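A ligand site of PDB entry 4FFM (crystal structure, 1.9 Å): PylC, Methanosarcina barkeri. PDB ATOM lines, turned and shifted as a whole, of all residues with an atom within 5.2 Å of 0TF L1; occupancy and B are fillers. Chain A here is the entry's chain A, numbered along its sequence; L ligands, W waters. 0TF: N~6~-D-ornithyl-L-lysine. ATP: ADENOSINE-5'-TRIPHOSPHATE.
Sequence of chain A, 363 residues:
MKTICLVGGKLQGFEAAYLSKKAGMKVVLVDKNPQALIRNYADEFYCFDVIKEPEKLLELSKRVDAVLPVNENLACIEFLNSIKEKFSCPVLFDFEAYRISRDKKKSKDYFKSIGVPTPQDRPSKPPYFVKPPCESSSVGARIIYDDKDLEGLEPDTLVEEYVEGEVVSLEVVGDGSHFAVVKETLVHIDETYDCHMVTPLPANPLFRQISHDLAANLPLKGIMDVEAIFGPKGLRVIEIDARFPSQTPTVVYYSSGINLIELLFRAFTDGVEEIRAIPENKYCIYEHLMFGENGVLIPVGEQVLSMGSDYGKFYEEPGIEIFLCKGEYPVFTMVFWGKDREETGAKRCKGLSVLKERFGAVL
Water W1 lies within hydrogen-bond range of O9 of 0TF L1 (2.7 Å) and O1B of ATP L2 (2.8 Å).
OD2 of Asp 225 lies within salt-bridge range of N17 of 0TF L1, 2.5 Å away.
OE1 of Gln 247 is in hydrogen-bond range of N13 of 0TF L1 (2.7 Å).
The side-chain carboxylate (OE1) of Glu 72 is in salt-bridge range of a nitrogen (N7) of 0TF L1 (2.8 Å).
The backbone NH (N) of Ser 246 lies within hydrogen-bond range of an oxygen (O18) of 0TF L1 (3.0 Å).
O of Ser 246 is in hydrogen-bond range of N13 of 0TF L1.
A nitrogen (N13) of 0TF L1 is in hydrogen-bond range of the side-chain hydroxyl (OG) of Ser 246, 3.2 Å away.
The backbone NH (N) of Gln 12 lies within hydrogen-bond range of an oxygen (O10) of 0TF L1.
The side-chain amide oxygen (OE1) of Gln 12 sits at hydrogen-bond distance from a nitrogen (N7) of 0TF L1 (2.9 Å).
OG1 of Thr 248 lies within hydrogen-bond range of N17 of 0TF L1, at 2.9 Å.
N17 of 0TF L1 lies within hydrogen-bond range of OG of Ser 169.
N of Leu 11 lies within hydrogen-bond range of O9 of 0TF L1, 3.0 Å away.
The side-chain carboxylate of Glu 302 is in salt-bridge range of a nitrogen (N13) of 0TF L1, 3.7 Å away.
N17 of 0TF L1 is in salt-bridge range of OE2 of Glu 171, at 3.1 Å.
An oxygen (O1A) of ATP L2 sits at hydrogen-bond distance from the backbone NH of Glu 72 (2.8 Å).
An oxygen (O1B) of ATP L2 is in salt-bridge range of the side-chain amino group (NZ) of Lys 10 (2.9 Å).
OD2 of Asp 225 sits at hydrogen-bond distance from OG of Ser 169 (3.2 Å).
The side-chain carboxylate of Glu 72 is in salt-bridge range of the guanidinium group of Arg 243 (2.9 Å).
OE1 of Glu 302 sits close to OG of Ser 246 (3.4 Å).
OE1 of Gln 12 sits close to N of Asn 71, at 3.4 Å.
The side-chain carboxylate (OE2) of Glu 171 is in hydrogen-bond range of the side-chain hydroxyl (OG1) of Thr 248, at 2.7 Å.
OG of Ser 169 lies within hydrogen-bond range of OE2 of Glu 171 (3.5 Å).
Residues that only touch 0TF L1: Lys 10 (3.0 Å), Pro 245 (3.5 Å), Arg 243 (3.6 Å) and Glu 227 (3.8 Å).
Hydrophobic or aromatic side chains within 4 Å of 0TF L1: Leu 11 and Pro 245.
Of the 19 residues printed, 14 come within 4 Å of 0TF L1.
A nitrogen (N7) of 0TF L1 lies within hydrogen-bond range of an oxygen (O1A) of ATP L2 (2.7 Å).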
ATOM      1  N   LYS A  10     -15.131  14.822 -24.691  1.00  0.00           N
ATOM      2  CA  LYS A  10     -15.555  16.129 -24.210  1.00  0.00           C
ATOM      3  C   LYS A  10     -14.525  17.220 -24.591  1.00  0.00           C
ATOM      4  O   LYS A  10     -14.149  17.317 -25.754  1.00  0.00           O
ATOM      5  CB  LYS A  10     -15.857  16.080 -22.703  1.00  0.00           C
ATOM      6  CG  LYS A  10     -17.340  16.011 -22.329  1.00  0.00           C
ATOM      7  CD  LYS A  10     -17.527  15.975 -20.822  1.00  0.00           C
ATOM      8  CE  LYS A  10     -18.679  16.857 -20.396  1.00  0.00           C
ATOM      9  NZ  LYS A  10     -19.089  16.641 -18.981  1.00  0.00           N
ATOM     10  N   LEU A  11     -14.066  18.035 -23.635  1.00  0.00           N
ATOM     11  CA  LEU A  11     -13.225  19.203 -23.960  1.00  0.00           C
ATOM     12  C   LEU A  11     -11.812  18.829 -24.426  1.00  0.00           C
ATOM     13  O   LEU A  11     -11.303  19.350 -25.435  1.00  0.00           O
ATOM     14  CB  LEU A  11     -13.163  20.200 -22.791  1.00  0.00           C
ATOM     15  CG  LEU A  11     -14.486  20.766 -22.266  1.00  0.00           C
ATOM     16  CD1 LEU A  11     -14.254  21.698 -21.068  1.00  0.00           C
ATOM     17  CD2 LEU A  11     -15.243  21.466 -23.382  1.00  0.00           C
ATOM     18  N   GLN A  12     -11.156  17.930 -23.691  1.00  0.00           N
ATOM     19  CA  GLN A  12      -9.825  17.462 -24.083  1.00  0.00           C
ATOM     20  C   GLN A  12      -9.941  16.720 -25.415  1.00  0.00           C
ATOM     21  O   GLN A  12      -9.086  16.867 -26.279  1.00  0.00           O
ATOM     22  CB  GLN A  12      -9.238  16.488 -23.069  1.00  0.00           C
ATOM     23  CG  GLN A  12      -8.926  16.990 -21.676  1.00  0.00           C
ATOM     24  CD  GLN A  12      -8.445  15.838 -20.811  1.00  0.00           C
ATOM     25  OE1 GLN A  12      -9.183  15.327 -19.979  1.00  0.00           O
ATOM     26  NE2 GLN A  12      -7.214  15.389 -21.049  1.00  0.00           N
ATOM     27  N   GLY A  13     -10.983  15.903 -25.545  1.00  0.00           N
ATOM     28  CA  GLY A  13     -11.234  15.144 -26.768  1.00  0.00           C
ATOM     29  C   GLY A  13     -11.437  16.050 -27.958  1.00  0.00           C
ATOM     30  O   GLY A  13     -10.899  15.784 -29.031  1.00  0.00           O
ATOM     31  N   VAL A  70      -7.936  10.945 -23.255  1.00  0.00           N
ATOM     32  CA  VAL A  70      -8.296  12.353 -23.109  1.00  0.00           C
ATOM     33  C   VAL A  70      -9.517  12.461 -22.174  1.00  0.00           C
ATOM     34  O   VAL A  70     -10.609  12.851 -22.592  1.00  0.00           O
ATOM     35  CB  VAL A  70      -8.480  13.077 -24.459  1.00  0.00           C
ATOM     36  CG1 VAL A  70      -7.172  13.678 -24.955  1.00  0.00           C
ATOM     37  CG2 VAL A  70      -9.096  12.173 -25.517  1.00  0.00           C
ATOM     38  N   ASN A  71      -9.296  12.050 -20.931  1.00  0.00           N
ATOM     39  CA  ASN A  71     -10.264  12.166 -19.837  1.00  0.00           C
ATOM     40  C   ASN A  71      -9.505  12.162 -18.517  1.00  0.00           C
ATOM     41  O   ASN A  71      -8.331  11.771 -18.458  1.00  0.00           O
ATOM     42  CB  ASN A  71     -11.352  11.062 -19.871  1.00  0.00           C
ATOM     43  CG  ASN A  71     -10.852   9.685 -19.468  1.00  0.00           C
ATOM     44  OD1 ASN A  71     -10.695   9.393 -18.290  1.00  0.00           O
ATOM     45  ND2 ASN A  71     -10.605   8.820 -20.456  1.00  0.00           N
ATOM     46  N   GLU A  72     -10.185  12.604 -17.471  1.00  0.00           N
ATOM     47  CA  GLU A  72      -9.625  12.697 -16.136  1.00  0.00           C
ATOM     48  C   GLU A  72     -10.512  11.887 -15.180  1.00  0.00           C
ATOM     49  O   GLU A  72     -10.688  12.247 -14.004  1.00  0.00           O
ATOM     50  CB  GLU A  72      -9.526  14.163 -15.700  1.00  0.00           C
ATOM     51  CG  GLU A  72      -8.685  15.033 -16.632  1.00  0.00           C
ATOM     52  CD  GLU A  72      -8.772  16.511 -16.315  1.00  0.00           C
ATOM     53  OE1 GLU A  72      -9.851  17.110 -16.526  1.00  0.00           O
ATOM     54  OE2 GLU A  72      -7.750  17.077 -15.881  1.00  0.00           O
ATOM     55  N   SER A 169       0.426  29.900 -19.155  1.00  0.00           N
ATOM     56  CA  SER A 169       0.528  28.476 -19.446  1.00  0.00           C
ATOM     57  C   SER A 169       1.668  28.129 -20.431  1.00  0.00           C
ATOM     58  O   SER A 169       1.962  28.877 -21.370  1.00  0.00           O
ATOM     59  CB  SER A 169      -0.826  27.984 -19.971  1.00  0.00           C
ATOM     60  OG  SER A 169      -0.756  26.660 -20.424  1.00  0.00           O
ATOM     61  N   GLU A 171       3.109  24.383 -22.383  1.00  0.00           N
ATOM     62  CA  GLU A 171       3.129  22.936 -22.584  1.00  0.00           C
ATOM     63  C   GLU A 171       4.556  22.478 -22.790  1.00  0.00           C
ATOM     64  O   GLU A 171       5.374  23.186 -23.369  1.00  0.00           O
ATOM     65  CB  GLU A 171       2.295  22.513 -23.790  1.00  0.00           C
ATOM     66  CG  GLU A 171       0.779  22.488 -23.576  1.00  0.00           C
ATOM     67  CD  GLU A 171       0.122  23.869 -23.558  1.00  0.00           C
ATOM     68  OE1 GLU A 171       0.503  24.769 -24.352  1.00  0.00           O
ATOM     69  OE2 GLU A 171      -0.806  24.063 -22.744  1.00  0.00           O
ATOM     70  N   VAL A 187      -3.793  32.939 -19.980  1.00  0.00           N
ATOM     71  CA  VAL A 187      -5.070  32.344 -19.614  1.00  0.00           C
ATOM     72  C   VAL A 187      -5.944  33.489 -19.046  1.00  0.00           C
ATOM     73  O   VAL A 187      -5.676  33.981 -17.961  1.00  0.00           O
ATOM     74  CB  VAL A 187      -4.856  31.192 -18.580  1.00  0.00           C
ATOM     75  CG1 VAL A 187      -6.178  30.634 -18.064  1.00  0.00           C
ATOM     76  CG2 VAL A 187      -4.020  30.060 -19.180  1.00  0.00           C
ATOM     77  N   ASP A 225       1.051  20.359 -19.097  1.00  0.00           N
ATOM     78  CA  ASP A 225       1.093  21.803 -19.067  1.00  0.00           C
ATOM     79  C   ASP A 225       1.492  22.285 -17.684  1.00  0.00           C
ATOM     80  O   ASP A 225       1.376  21.563 -16.690  1.00  0.00           O
ATOM     81  CB  ASP A 225      -0.177  22.453 -19.635  1.00  0.00           C
ATOM     82  CG  ASP A 225      -1.082  22.971 -18.571  1.00  0.00           C
ATOM     83  OD1 ASP A 225      -1.421  22.208 -17.651  1.00  0.00           O
ATOM     84  OD2 ASP A 225      -1.479  24.129 -18.674  1.00  0.00           O
ATOM     85  N   GLU A 227       1.103  25.740 -15.246  1.00  0.00           N
ATOM     86  CA  GLU A 227       0.464  27.041 -15.063  1.00  0.00           C
ATOM     87  C   GLU A 227       1.145  27.782 -13.924  1.00  0.00           C
ATOM     88  O   GLU A 227       1.367  27.218 -12.847  1.00  0.00           O
ATOM     89  CB  GLU A 227      -1.047  26.962 -14.760  1.00  0.00           C
ATOM     90  CG  GLU A 227      -1.881  25.935 -15.517  1.00  0.00           C
ATOM     91  CD  GLU A 227      -3.411  26.141 -15.360  1.00  0.00           C
ATOM     92  OE1 GLU A 227      -4.114  25.616 -14.388  1.00  0.00           O
ATOM     93  OE2 GLU A 227      -3.936  26.851 -16.245  1.00  0.00           O
ATOM     94  N   ARG A 243      -1.650  15.733 -18.916  1.00  0.00           N
ATOM     95  CA  ARG A 243      -2.701  15.217 -19.777  1.00  0.00           C
ATOM     96  C   ARG A 243      -2.892  16.227 -20.915  1.00  0.00           C
ATOM     97  O   ARG A 243      -2.515  17.387 -20.763  1.00  0.00           O
ATOM     98  CB  ARG A 243      -4.004  14.945 -18.990  1.00  0.00           C
ATOM     99  CG  ARG A 243      -4.471  16.055 -18.028  1.00  0.00           C
ATOM    100  CD  ARG A 243      -5.290  17.110 -18.766  1.00  0.00           C
ATOM    101  NE  ARG A 243      -5.928  18.116 -17.909  1.00  0.00           N
ATOM    102  CZ  ARG A 243      -5.620  19.417 -17.907  1.00  0.00           C
ATOM    103  NH1 ARG A 243      -4.674  19.880 -18.698  1.00  0.00           N
ATOM    104  NH2 ARG A 243      -6.263  20.248 -17.098  1.00  0.00           N
ATOM    105  N   PRO A 245      -4.198  19.126 -22.875  1.00  0.00           N
ATOM    106  CA  PRO A 245      -5.084  20.226 -22.463  1.00  0.00           C
ATOM    107  C   PRO A 245      -6.090  20.686 -23.518  1.00  0.00           C
ATOM    108  O   PRO A 245      -5.978  20.323 -24.693  1.00  0.00           O
ATOM    109  CB  PRO A 245      -4.112  21.383 -22.188  1.00  0.00           C
ATOM    110  CG  PRO A 245      -2.947  21.102 -23.048  1.00  0.00           C
ATOM    111  CD  PRO A 245      -2.817  19.608 -23.153  1.00  0.00           C
ATOM    112  N   SER A 246      -7.054  21.499 -23.105  1.00  0.00           N
ATOM    113  CA  SER A 246      -7.935  22.192 -24.028  1.00  0.00           C
ATOM    114  C   SER A 246      -7.520  23.667 -24.143  1.00  0.00           C
ATOM    115  O   SER A 246      -6.789  24.170 -23.269  1.00  0.00           O
ATOM    116  CB  SER A 246      -9.375  22.096 -23.563  1.00  0.00           C
ATOM    117  OG  SER A 246      -9.503  22.749 -22.311  1.00  0.00           O
ATOM    118  N   GLN A 247      -7.970  24.330 -25.220  1.00  0.00           N
ATOM    119  CA  GLN A 247      -7.836  25.787 -25.435  1.00  0.00           C
ATOM    120  C   GLN A 247      -6.444  26.229 -25.850  1.00  0.00           C
ATOM    121  O   GLN A 247      -6.260  26.719 -26.952  1.00  0.00           O
ATOM    122  CB  GLN A 247      -8.298  26.605 -24.212  1.00  0.00           C
ATOM    123  CG  GLN A 247      -9.639  26.195 -23.608  1.00  0.00           C
ATOM    124  CD  GLN A 247      -9.995  27.038 -22.402  1.00  0.00           C
ATOM    125  OE1 GLN A 247      -9.259  27.066 -21.412  1.00  0.00           O
ATOM    126  NE2 GLN A 247     -11.132  27.713 -22.469  1.00  0.00           N
ATOM    127  N   THR A 248      -5.461  26.040 -24.968  1.00  0.00           N
ATOM    128  CA  THR A 248      -4.123  26.534 -25.235  1.00  0.00           C
ATOM    129  C   THR A 248      -3.456  25.915 -26.492  1.00  0.00           C
ATOM    130  O   THR A 248      -2.753  26.630 -27.211  1.00  0.00           O
ATOM    131  CB  THR A 248      -3.200  26.462 -23.987  1.00  0.00           C
ATOM    132  OG1 THR A 248      -3.151  25.125 -23.489  1.00  0.00           O
ATOM    133  CG2 THR A 248      -3.690  27.388 -22.862  1.00  0.00           C
ATOM    134  N   GLU A 302     -14.967  27.472 -20.082  1.00  0.00           N
ATOM    135  CA  GLU A 302     -15.022  26.062 -20.464  1.00  0.00           C
ATOM    136  C   GLU A 302     -16.122  25.228 -19.836  1.00  0.00           C
ATOM    137  O   GLU A 302     -16.676  24.353 -20.503  1.00  0.00           O
ATOM    138  CB  GLU A 302     -13.758  25.379 -19.976  1.00  0.00           C
ATOM    139  CG  GLU A 302     -12.536  25.680 -20.755  1.00  0.00           C
ATOM    140  CD  GLU A 302     -11.660  24.482 -20.797  1.00  0.00           C
ATOM    141  OE1 GLU A 302     -11.235  24.024 -19.707  1.00  0.00           O
ATOM    142  OE2 GLU A 302     -11.452  23.983 -21.910  1.00  0.00           O
ATOM    143  N   SER A 306     -18.883  22.570 -21.550  1.00  0.00           N
ATOM    144  CA  SER A 306     -18.916  21.147 -21.253  1.00  0.00           C
ATOM    145  C   SER A 306     -20.322  20.646 -20.892  1.00  0.00           C
ATOM    146  O   SER A 306     -20.498  19.461 -20.648  1.00  0.00           O
ATOM    147  CB  SER A 306     -17.987  20.830 -20.103  1.00  0.00           C
ATOM    148  OG  SER A 306     -18.661  21.120 -18.886  1.00  0.00           O
HETATM  149  O18 0TF L   1      -6.941  22.256 -20.237  1.00  0.00           O
HETATM  150  C11 0TF L   1      -7.790  22.813 -19.567  1.00  0.00           C
HETATM  151  C12 0TF L   1      -7.671  24.309 -19.352  1.00  0.00           C
HETATM  152  C14 0TF L   1      -6.295  24.745 -18.766  1.00  0.00           C
HETATM  153  C15 0TF L   1      -5.235  24.664 -19.916  1.00  0.00           C
HETATM  154  C16 0TF L   1      -3.910  25.442 -19.754  1.00  0.00           C
HETATM  155  N17 0TF L   1      -2.932  24.764 -20.637  1.00  0.00           N
HETATM  156  N13 0TF L   1      -7.772  24.892 -20.697  1.00  0.00           N
HETATM  157  N6  0TF L   1      -8.891  22.162 -19.110  1.00  0.00           N
HETATM  158  C5  0TF L   1      -9.204  20.787 -19.480  1.00  0.00           C
HETATM  159  C4  0TF L   1     -10.562  20.417 -18.826  1.00  0.00           C
HETATM  160  C3  0TF L   1     -11.116  19.088 -19.395  1.00  0.00           C
HETATM  161  C2  0TF L   1     -12.255  18.532 -18.503  1.00  0.00           C
HETATM  162  C1  0TF L   1     -12.642  17.079 -18.881  1.00  0.00           C
HETATM  163  N7  0TF L   1     -11.552  16.130 -18.584  1.00  0.00           N
HETATM  164  C8  0TF L   1     -13.033  17.006 -20.340  1.00  0.00           C
HETATM  165  O10 0TF L   1     -12.280  16.414 -21.148  1.00  0.00           O
HETATM  166  O9  0TF L   1     -14.101  17.562 -20.701  1.00  0.00           O
HETATM  167  PG  ATP L   2     -18.595  13.176 -16.641  1.00  0.00           P
HETATM  168  O1G ATP L   2     -19.899  13.877 -16.946  1.00  0.00           O
HETATM  169  O2G ATP L   2     -18.209  13.240 -15.181  1.00  0.00           O
HETATM  170  O3G ATP L   2     -18.517  11.786 -17.247  1.00  0.00           O
HETATM  171  PB  ATP L   2     -16.355  15.030 -16.872  1.00  0.00           P
HETATM  172  O1B ATP L   2     -16.725  16.434 -17.286  1.00  0.00           O
HETATM  173  O2B ATP L   2     -16.021  14.724 -15.424  1.00  0.00           O
HETATM  174  O3B ATP L   2     -17.462  14.004 -17.468  1.00  0.00           O
HETATM  175  PA  ATP L   2     -14.152  13.315 -17.656  1.00  0.00           P
HETATM  176  O1A ATP L   2     -12.719  13.736 -17.951  1.00  0.00           O
HETATM  177  O2A ATP L   2     -14.456  12.384 -16.511  1.00  0.00           O
HETATM  178  O3A ATP L   2     -15.034  14.665 -17.722  1.00  0.00           O
HETATM  179  O5' ATP L   2     -14.594  12.529 -18.977  1.00  0.00           O
HETATM  180  C5' ATP L   2     -14.508  13.120 -20.278  1.00  0.00           C
HETATM  181  C4' ATP L   2     -15.122  12.178 -21.292  1.00  0.00           C
HETATM  182  O4' ATP L   2     -14.454  10.917 -21.174  1.00  0.00           O
HETATM  183  C3' ATP L   2     -16.596  11.959 -20.984  1.00  0.00           C
HETATM  184  O3' ATP L   2     -17.345  12.216 -22.178  1.00  0.00           O
HETATM  185  C2' ATP L   2     -16.670  10.514 -20.540  1.00  0.00           C
HETATM  186  O2' ATP L   2     -17.914   9.860 -20.861  1.00  0.00           O
HETATM  187  C1' ATP L   2     -15.410   9.864 -21.137  1.00  0.00           C
HETATM  188  N9  ATP L   2     -15.014   8.689 -20.312  1.00  0.00           N
HETATM  189  C8  ATP L   2     -14.685   8.698 -19.000  1.00  0.00           C
HETATM  190  N7  ATP L   2     -14.429   7.445 -18.551  1.00  0.00           N
HETATM  191  C5  ATP L   2     -14.604   6.603 -19.592  1.00  0.00           C
HETATM  192  C6  ATP L   2     -14.492   5.132 -19.809  1.00  0.00           C
HETATM  193  N6  ATP L   2     -14.158   4.289 -18.794  1.00  0.00           N
HETATM  194  N1  ATP L   2     -14.753   4.686 -21.061  1.00  0.00           N
HETATM  195  C2  ATP L   2     -15.109   5.482 -22.082  1.00  0.00           C
HETATM  196  N3  ATP L   2     -15.234   6.821 -21.949  1.00  0.00           N
HETATM  197  C4  ATP L   2     -14.989   7.422 -20.754  1.00  0.00           C
HETATM  198  O   HOH W   1     -15.720  18.625 -18.804  1.00  0.00           O
HETATM  199  O   HOH W   2      -8.159  26.804 -16.963  1.00  0.00           O
HETATM  200  O   HOH W   3      -5.840  24.337 -15.672  1.00  0.00           O
HETATM  201  O   HOH W   4     -12.579  14.843 -23.222  1.00  0.00           O
